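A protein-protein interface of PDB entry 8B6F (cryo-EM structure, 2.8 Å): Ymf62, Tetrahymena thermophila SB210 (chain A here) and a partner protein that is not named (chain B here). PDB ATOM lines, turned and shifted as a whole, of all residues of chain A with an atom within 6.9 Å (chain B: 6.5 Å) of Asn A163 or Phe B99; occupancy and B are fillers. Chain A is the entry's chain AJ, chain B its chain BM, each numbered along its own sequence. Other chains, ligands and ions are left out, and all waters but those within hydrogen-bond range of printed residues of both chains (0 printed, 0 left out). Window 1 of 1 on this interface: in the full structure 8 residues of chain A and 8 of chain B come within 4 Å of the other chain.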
ATOM      1  N   TYR A 158      -1.164  -1.731 -10.484  1.00  0.00           N
ATOM      2  CA  TYR A 158       0.131  -2.307 -10.142  1.00  0.00           C
ATOM      3  C   TYR A 158       0.483  -2.087  -8.678  1.00  0.00           C
ATOM      4  O   TYR A 158       1.150  -2.933  -8.073  1.00  0.00           O
ATOM      5  CB  TYR A 158       1.216  -1.729 -11.048  1.00  0.00           C
ATOM      6  CG  TYR A 158       1.033  -2.119 -12.492  1.00  0.00           C
ATOM      7  CD1 TYR A 158       0.236  -1.366 -13.339  1.00  0.00           C
ATOM      8  CD2 TYR A 158       1.646  -3.255 -13.005  1.00  0.00           C
ATOM      9  CE1 TYR A 158       0.059  -1.724 -14.656  1.00  0.00           C
ATOM     10  CE2 TYR A 158       1.476  -3.623 -14.321  1.00  0.00           C
ATOM     11  CZ  TYR A 158       0.681  -2.853 -15.142  1.00  0.00           C
ATOM     12  OH  TYR A 158       0.507  -3.216 -16.454  1.00  0.00           O
ATOM     13  N   TYR A 159       0.054  -0.969  -8.091  1.00  0.00           N
ATOM     14  CA  TYR A 159       0.303  -0.750  -6.670  1.00  0.00           C
ATOM     15  C   TYR A 159      -0.386  -1.816  -5.830  1.00  0.00           C
ATOM     16  O   TYR A 159       0.228  -2.422  -4.945  1.00  0.00           O
ATOM     17  CB  TYR A 159      -0.150   0.649  -6.261  1.00  0.00           C
ATOM     18  CG  TYR A 159       0.880   1.713  -6.556  1.00  0.00           C
ATOM     19  CD1 TYR A 159       0.925   2.343  -7.792  1.00  0.00           C
ATOM     20  CD2 TYR A 159       1.820   2.073  -5.602  1.00  0.00           C
ATOM     21  CE1 TYR A 159       1.872   3.312  -8.062  1.00  0.00           C
ATOM     22  CE2 TYR A 159       2.768   3.039  -5.860  1.00  0.00           C
ATOM     23  CZ  TYR A 159       2.791   3.654  -7.092  1.00  0.00           C
ATOM     24  OH  TYR A 159       3.736   4.616  -7.349  1.00  0.00           O
ATOM     25  N   GLU A 160      -1.672  -2.051  -6.086  1.00  0.00           N
ATOM     26  CA  GLU A 160      -2.372  -3.131  -5.403  1.00  0.00           C
ATOM     27  C   GLU A 160      -1.767  -4.483  -5.751  1.00  0.00           C
ATOM     28  O   GLU A 160      -1.754  -5.391  -4.914  1.00  0.00           O
ATOM     29  CB  GLU A 160      -3.859  -3.100  -5.757  1.00  0.00           C
ATOM     30  CG  GLU A 160      -4.734  -3.990  -4.880  1.00  0.00           C
ATOM     31  CD  GLU A 160      -4.698  -5.453  -5.285  1.00  0.00           C
ATOM     32  OE1 GLU A 160      -4.238  -5.752  -6.407  1.00  0.00           O
ATOM     33  OE2 GLU A 160      -5.137  -6.303  -4.483  1.00  0.00           O
ATOM     34  N   GLY A 161      -1.266  -4.636  -6.977  1.00  0.00           N
ATOM     35  CA  GLY A 161      -0.656  -5.898  -7.361  1.00  0.00           C
ATOM     36  C   GLY A 161       0.564  -6.240  -6.528  1.00  0.00           C
ATOM     37  O   GLY A 161       0.705  -7.365  -6.046  1.00  0.00           O
ATOM     38  N   PHE A 162       1.462  -5.273  -6.342  1.00  0.00           N
ATOM     39  CA  PHE A 162       2.655  -5.531  -5.545  1.00  0.00           C
ATOM     40  C   PHE A 162       2.369  -5.529  -4.051  1.00  0.00           C
ATOM     41  O   PHE A 162       3.164  -6.084  -3.284  1.00  0.00           O
ATOM     42  CB  PHE A 162       3.751  -4.513  -5.888  1.00  0.00           C
ATOM     43  CG  PHE A 162       3.816  -3.336  -4.956  1.00  0.00           C
ATOM     44  CD1 PHE A 162       4.507  -3.408  -3.758  1.00  0.00           C
ATOM     45  CD2 PHE A 162       3.233  -2.136  -5.312  1.00  0.00           C
ATOM     46  CE1 PHE A 162       4.575  -2.316  -2.916  1.00  0.00           C
ATOM     47  CE2 PHE A 162       3.297  -1.038  -4.477  1.00  0.00           C
ATOM     48  CZ  PHE A 162       3.970  -1.128  -3.277  1.00  0.00           C
ATOM     49  N   ASN A 163       1.262  -4.929  -3.619  1.00  0.00           N
ATOM     50  CA  ASN A 163       0.835  -5.046  -2.231  1.00  0.00           C
ATOM     51  C   ASN A 163       0.070  -6.332  -1.958  1.00  0.00           C
ATOM     52  O   ASN A 163      -0.168  -6.654  -0.789  1.00  0.00           O
ATOM     53  CB  ASN A 163      -0.042  -3.852  -1.843  1.00  0.00           C
ATOM     54  CG  ASN A 163       0.752  -2.573  -1.683  1.00  0.00           C
ATOM     55  OD1 ASN A 163       0.466  -1.568  -2.336  1.00  0.00           O
ATOM     56  ND2 ASN A 163       1.754  -2.601  -0.814  1.00  0.00           N
ATOM     57  N   ASN A 164      -0.321  -7.069  -2.994  1.00  0.00           N
ATOM     58  CA  ASN A 164      -1.086  -8.295  -2.829  1.00  0.00           C
ATOM     59  C   ASN A 164      -0.137  -9.481  -2.719  1.00  0.00           C
ATOM     60  O   ASN A 164       0.730  -9.673  -3.578  1.00  0.00           O
ATOM     61  CB  ASN A 164      -2.040  -8.485  -4.009  1.00  0.00           C
ATOM     62  CG  ASN A 164      -3.051  -9.585  -3.772  1.00  0.00           C
ATOM     63  OD1 ASN A 164      -2.799 -10.523  -3.018  1.00  0.00           O
ATOM     64  ND2 ASN A 164      -4.205  -9.477  -4.417  1.00  0.00           N
ATOM     65  N   SER A 165      -0.305 -10.275  -1.664  1.00  0.00           N
ATOM     66  CA  SER A 165       0.526 -11.445  -1.422  1.00  0.00           C
ATOM     67  C   SER A 165      -0.230 -12.757  -1.579  1.00  0.00           C
ATOM     68  O   SER A 165       0.346 -13.821  -1.328  1.00  0.00           O
ATOM     69  CB  SER A 165       1.143 -11.369  -0.021  1.00  0.00           C
ATOM     70  OG  SER A 165       0.136 -11.335   0.977  1.00  0.00           O
ATOM     71  N   ILE A 166      -1.498 -12.715  -1.986  1.00  0.00           N
ATOM     72  CA  ILE A 166      -2.288 -13.932  -2.107  1.00  0.00           C
ATOM     73  C   ILE A 166      -1.765 -14.780  -3.260  1.00  0.00           C
ATOM     74  O   ILE A 166      -1.291 -14.264  -4.281  1.00  0.00           O
ATOM     75  CB  ILE A 166      -3.775 -13.581  -2.298  1.00  0.00           C
ATOM     76  CG1 ILE A 166      -4.299 -12.824  -1.075  1.00  0.00           C
ATOM     77  CG2 ILE A 166      -4.604 -14.837  -2.537  1.00  0.00           C
ATOM     78  CD1 ILE A 166      -5.619 -12.130  -1.307  1.00  0.00           C
ATOM     79  N   GLN B  97      -2.574 -10.497   9.276  1.00  0.00           N
ATOM     80  CA  GLN B  97      -3.393 -10.867   8.136  1.00  0.00           C
ATOM     81  C   GLN B  97      -3.190  -9.873   7.004  1.00  0.00           C
ATOM     82  O   GLN B  97      -2.738  -8.746   7.231  1.00  0.00           O
ATOM     83  CB  GLN B  97      -4.878 -10.932   8.525  1.00  0.00           C
ATOM     84  CG  GLN B  97      -5.200 -12.065   9.493  1.00  0.00           C
ATOM     85  CD  GLN B  97      -6.651 -12.072   9.934  1.00  0.00           C
ATOM     86  OE1 GLN B  97      -7.292 -11.026  10.011  1.00  0.00           O
ATOM     87  NE2 GLN B  97      -7.175 -13.255  10.224  1.00  0.00           N
ATOM     88  N   PRO B  98      -3.507 -10.263   5.769  1.00  0.00           N
ATOM     89  CA  PRO B  98      -3.251  -9.388   4.617  1.00  0.00           C
ATOM     90  C   PRO B  98      -3.950  -8.043   4.748  1.00  0.00           C
ATOM     91  O   PRO B  98      -4.782  -7.812   5.627  1.00  0.00           O
ATOM     92  CB  PRO B  98      -3.795 -10.190   3.431  1.00  0.00           C
ATOM     93  CG  PRO B  98      -3.765 -11.599   3.882  1.00  0.00           C
ATOM     94  CD  PRO B  98      -4.046 -11.569   5.351  1.00  0.00           C
ATOM     95  N   PHE B  99      -3.595  -7.138   3.832  1.00  0.00           N
ATOM     96  CA  PHE B  99      -4.158  -5.792   3.864  1.00  0.00           C
ATOM     97  C   PHE B  99      -5.665  -5.820   3.644  1.00  0.00           C
ATOM     98  O   PHE B  99      -6.406  -5.057   4.274  1.00  0.00           O
ATOM     99  CB  PHE B  99      -3.481  -4.906   2.821  1.00  0.00           C
ATOM    100  CG  PHE B  99      -3.878  -5.218   1.410  1.00  0.00           C
ATOM    101  CD1 PHE B  99      -3.261  -6.241   0.714  1.00  0.00           C
ATOM    102  CD2 PHE B  99      -4.865  -4.482   0.777  1.00  0.00           C
ATOM    103  CE1 PHE B  99      -3.626  -6.528  -0.585  1.00  0.00           C
ATOM    104  CE2 PHE B  99      -5.235  -4.763  -0.521  1.00  0.00           C
ATOM    105  CZ  PHE B  99      -4.614  -5.787  -1.204  1.00  0.00           C
ATOM    106  N   GLY B 100      -6.140  -6.685   2.749  1.00  0.00           N
ATOM    107  CA  GLY B 100      -7.572  -6.795   2.539  1.00  0.00           C
ATOM    108  C   GLY B 100      -8.311  -7.160   3.812  1.00  0.00           C
ATOM    109  O   GLY B 100      -9.363  -6.596   4.115  1.00  0.00           O
ATOM    110  N   HIS B 101      -7.765  -8.109   4.576  1.00  0.00           N
ATOM    111  CA  HIS B 101      -8.353  -8.451   5.865  1.00  0.00           C
ATOM    112  C   HIS B 101      -8.302  -7.266   6.819  1.00  0.00           C
ATOM    113  O   HIS B 101      -9.322  -6.864   7.387  1.00  0.00           O
ATOM    114  CB  HIS B 101      -7.616  -9.645   6.476  1.00  0.00           C
ATOM    115  CG  HIS B 101      -7.790 -10.926   5.720  1.00  0.00           C
ATOM    116  ND1 HIS B 101      -8.122 -12.113   6.338  1.00  0.00           N
ATOM    117  CD2 HIS B 101      -7.672 -11.208   4.402  1.00  0.00           C
ATOM    118  CE1 HIS B 101      -8.202 -13.071   5.432  1.00  0.00           C
ATOM    119  NE2 HIS B 101      -7.934 -12.549   4.248  1.00  0.00           N
ATOM    120  N   THR B 102      -7.118  -6.680   6.996  1.00  0.00           N
ATOM    121  CA  THR B 102      -6.933  -5.712   8.073  1.00  0.00           C
ATOM    122  C   THR B 102      -7.756  -4.451   7.839  1.00  0.00           C
ATOM    123  O   THR B 102      -8.303  -3.882   8.790  1.00  0.00           O
ATOM    124  CB  THR B 102      -5.446  -5.378   8.232  1.00  0.00           C
ATOM    125  OG1 THR B 102      -5.231  -4.747   9.499  1.00  0.00           O
ATOM    126  CG2 THR B 102      -4.971  -4.432   7.146  1.00  0.00           C
ATOM    127  N   PHE B 103      -7.847  -3.986   6.591  1.00  0.00           N
ATOM    128  CA  PHE B 103      -8.608  -2.769   6.327  1.00  0.00           C
ATOM    129  C   PHE B 103     -10.070  -2.935   6.715  1.00  0.00           C
ATOM    130  O   PHE B 103     -10.633  -2.102   7.433  1.00  0.00           O
ATOM    131  CB  PHE B 103      -8.505  -2.378   4.854  1.00  0.00           C
ATOM    132  CG  PHE B 103      -9.386  -1.223   4.487  1.00  0.00           C
ATOM    133  CD1 PHE B 103      -8.981   0.077   4.731  1.00  0.00           C
ATOM    134  CD2 PHE B 103     -10.630  -1.437   3.920  1.00  0.00           C
ATOM    135  CE1 PHE B 103      -9.792   1.142   4.409  1.00  0.00           C
ATOM    136  CE2 PHE B 103     -11.449  -0.375   3.595  1.00  0.00           C
ATOM    137  CZ  PHE B 103     -11.028   0.916   3.838  1.00  0.00           C
ATOM    138  N   VAL B 104     -10.704  -4.010   6.250  1.00  0.00           N
ATOM    139  CA  VAL B 104     -12.114  -4.222   6.554  1.00  0.00           C
ATOM    140  C   VAL B 104     -12.305  -4.469   8.043  1.00  0.00           C
ATOM    141  O   VAL B 104     -13.309  -4.051   8.632  1.00  0.00           O
ATOM    142  CB  VAL B 104     -12.671  -5.382   5.710  1.00  0.00           C
ATOM    143  CG1 VAL B 104     -14.132  -5.646   6.055  1.00  0.00           C
ATOM    144  CG2 VAL B 104     -12.522  -5.077   4.229  1.00  0.00           C
ATOM    145  N   TRP B 117      -5.534   5.379   6.125  1.00  0.00           N
ATOM    146  CA  TRP B 117      -5.039   4.244   5.358  1.00  0.00           C
ATOM    147  C   TRP B 117      -4.075   4.734   4.287  1.00  0.00           C
ATOM    148  O   TRP B 117      -4.390   5.664   3.538  1.00  0.00           O
ATOM    149  CB  TRP B 117      -6.196   3.475   4.715  1.00  0.00           C
ATOM    150  CG  TRP B 117      -5.769   2.294   3.894  1.00  0.00           C
ATOM    151  CD1 TRP B 117      -5.543   2.271   2.550  1.00  0.00           C
ATOM    152  CD2 TRP B 117      -5.526   0.963   4.364  1.00  0.00           C
ATOM    153  NE1 TRP B 117      -5.172   1.010   2.153  1.00  0.00           N
ATOM    154  CE2 TRP B 117      -5.154   0.188   3.249  1.00  0.00           C
ATOM    155  CE3 TRP B 117      -5.585   0.353   5.620  1.00  0.00           C
ATOM    156  CZ2 TRP B 117      -4.842  -1.165   3.353  1.00  0.00           C
ATOM    157  CZ3 TRP B 117      -5.276  -0.992   5.721  1.00  0.00           C
ATOM    158  CH2 TRP B 117      -4.909  -1.736   4.593  1.00  0.00           C
ATOM    159  N   ASN B 118      -2.905   4.105   4.219  1.00  0.00           N
ATOM    160  CA  ASN B 118      -1.917   4.415   3.193  1.00  0.00           C
ATOM    161  C   ASN B 118      -2.271   3.628   1.938  1.00  0.00           C
ATOM    162  O   ASN B 118      -2.088   2.408   1.889  1.00  0.00           O
ATOM    163  CB  ASN B 118      -0.516   4.071   3.689  1.00  0.00           C
ATOM    164  CG  ASN B 118       0.549   4.949   3.079  1.00  0.00           C
ATOM    165  OD1 ASN B 118       0.905   4.793   1.915  1.00  0.00           O
ATOM    166  ND2 ASN B 118       1.077   5.874   3.871  1.00  0.00           N
ATOM    167  N   HIS B 119      -2.781   4.322   0.919  1.00  0.00           N
ATOM    168  CA  HIS B 119      -3.325   3.631  -0.246  1.00  0.00           C
ATOM    169  C   HIS B 119      -2.246   2.856  -0.992  1.00  0.00           C
ATOM    170  O   HIS B 119      -2.403   1.660  -1.264  1.00  0.00           O
ATOM    171  CB  HIS B 119      -3.998   4.635  -1.180  1.00  0.00           C
ATOM    172  CG  HIS B 119      -4.357   4.064  -2.514  1.00  0.00           C
ATOM    173  ND1 HIS B 119      -5.254   3.028  -2.663  1.00  0.00           N
ATOM    174  CD2 HIS B 119      -3.935   4.379  -3.760  1.00  0.00           C
ATOM    175  CE1 HIS B 119      -5.369   2.732  -3.945  1.00  0.00           C
ATOM    176  NE2 HIS B 119      -4.580   3.537  -4.632  1.00  0.00           N
ATOM    177  N   ASN B 120      -1.143   3.517  -1.332  1.00  0.00           N
ATOM    178  CA  ASN B 120      -0.128   2.887  -2.168  1.00  0.00           C
ATOM    179  C   ASN B 120       0.761   1.921  -1.401  1.00  0.00           C
ATOM    180  O   ASN B 120       1.551   1.208  -2.027  1.00  0.00           O
ATOM    181  CB  ASN B 120       0.732   3.953  -2.851  1.00  0.00           C
ATOM    182  CG  ASN B 120       1.292   4.963  -1.877  1.00  0.00           C
ATOM    183  OD1 ASN B 120       1.326   4.727  -0.672  1.00  0.00           O
ATOM    184  ND2 ASN B 120       1.734   6.101  -2.397  1.00  0.00           N
ATOM    185  N   PHE B 121       0.659   1.878  -0.071  1.00  0.00           N
ATOM    186  CA  PHE B 121       1.378   0.899   0.728  1.00  0.00           C
ATOM    187  C   PHE B 121       0.466  -0.051   1.485  1.00  0.00           C
ATOM    188  O   PHE B 121       0.968  -0.990   2.113  1.00  0.00           O
ATOM    189  CB  PHE B 121       2.316   1.600   1.724  1.00  0.00           C
ATOM    190  CG  PHE B 121       3.524   2.207   1.077  1.00  0.00           C
ATOM    191  CD1 PHE B 121       4.564   1.405   0.642  1.00  0.00           C
ATOM    192  CD2 PHE B 121       3.617   3.576   0.896  1.00  0.00           C
ATOM    193  CE1 PHE B 121       5.678   1.956   0.042  1.00  0.00           C
ATOM    194  CE2 PHE B 121       4.727   4.134   0.297  1.00  0.00           C
ATOM    195  CZ  PHE B 121       5.760   3.322  -0.131  1.00  0.00           C
ATOM    196  N   ALA B 122      -0.848   0.156   1.443  1.00  0.00           N
ATOM    197  CA  ALA B 122      -1.821  -0.788   1.984  1.00  0.00           C
ATOM    198  C   ALA B 122      -1.564  -1.071   3.464  1.00  0.00           C
ATOM    199  O   ALA B 122      -1.292  -2.202   3.874  1.00  0.00           O
ATOM    200  CB  ALA B 122      -1.816  -2.085   1.169  1.00  0.00           C
ATOM    201  N   CYS B 123      -1.658  -0.017   4.268  1.00  0.00           N
ATOM    202  CA  CYS B 123      -1.519  -0.150   5.713  1.00  0.00           C
ATOM    203  C   CYS B 123      -1.983   1.138   6.369  1.00  0.00           C
ATOM    204  O   CYS B 123      -2.066   2.189   5.727  1.00  0.00           O
ATOM    205  CB  CYS B 123      -0.077  -0.469   6.116  1.00  0.00           C
ATOM    206  SG  CYS B 123       1.167   0.561   5.313  1.00  0.00           S
ATOM    207  N   TYR B 124      -2.286   1.041   7.660  1.00  0.00           N
ATOM    208  CA  TYR B 124      -2.699   2.199   8.430  1.00  0.00           C
ATOM    209  C   TYR B 124      -1.482   2.967   8.937  1.00  0.00           C
ATOM    210  O   TYR B 124      -0.360   2.458   8.968  1.00  0.00           O
ATOM    211  CB  TYR B 124      -3.574   1.782   9.611  1.00  0.00           C
ATOM    212  CG  TYR B 124      -4.960   1.319   9.227  1.00  0.00           C
ATOM    213  CD1 TYR B 124      -5.964   2.235   8.949  1.00  0.00           C
ATOM    214  CD2 TYR B 124      -5.266  -0.032   9.155  1.00  0.00           C
ATOM    215  CE1 TYR B 124      -7.233   1.820   8.606  1.00  0.00           C
ATOM    216  CE2 TYR B 124      -6.534  -0.457   8.811  1.00  0.00           C
ATOM    217  CZ  TYR B 124      -7.513   0.475   8.540  1.00  0.00           C
ATOM    218  OH  TYR B 124      -8.778   0.064   8.198  1.00  0.00           O
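O of Asn B120 sits close to OD1 of Asn A163 (3.0 Å). The backbone carbonyl oxygen of Phe B121 is in hydrogen-bond range of the side-chain amide nitrogen of Asn A163 (3.4 Å).
Of the 9 printed residues of chain A, 5 touch a printed residue of chain B. Hydrophobic or aromatic side chains of chain A that line the printed part of chain B: Tyr A159 and Phe A162. Along chain A the printed residues that touch a printed residue of chain B span positions 159 to 164. Among the printed residues, no Asp or Glu carboxylate lies within 4 Å of a Lys or Arg side-chain nitrogen of the other chain.
The backbone carbonyl oxygen of Tyr A159 lies close to the side-chain amide oxygen of Asn A163, at 2.8 Å. The side-chain amide nitrogen (ND2) of Asn A164 lies within hydrogen-bond range of the side-chain carboxylate (OE2) of Glu A160, at 3.3 Å. The side-chain amide oxygen (OD1) of Asn A164 lies within hydrogen-bond range of the backbone NH (N) of Ile A166, 2.7 Å away. OD1 of Asn B120 lies close to OD1 of Asn B118, at 2.6 Å.
Asn B120 touches Tyr A159. Glu A160 touches Phe B99 (OE2 to CZ, 3.4 Å). Phe A162 touches Asn B120. O of Asn A163 touches CD1 of Phe B99 (3.5 Å). Asn A163 touches Ala B122. CA of Asn A164 touches CE1 of Phe B99, at 3.8 Å.
Of the printed residues of chain B, Glu A160 touches Phe B99. Asn A163 touches four residues of chain B. Printed residues of chain B within 4 Å of Asn A164: Phe B99. Of chain A, only Glu A160, Asn A163 and Asn A164 come within 4 Å of Phe B99. The nearest residue of chain B that does not touch Asn A163 is His B119 (4.4 Å). The nearest residue of chain A that does not touch Phe B99 is Ser A165 (5.1 Å).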
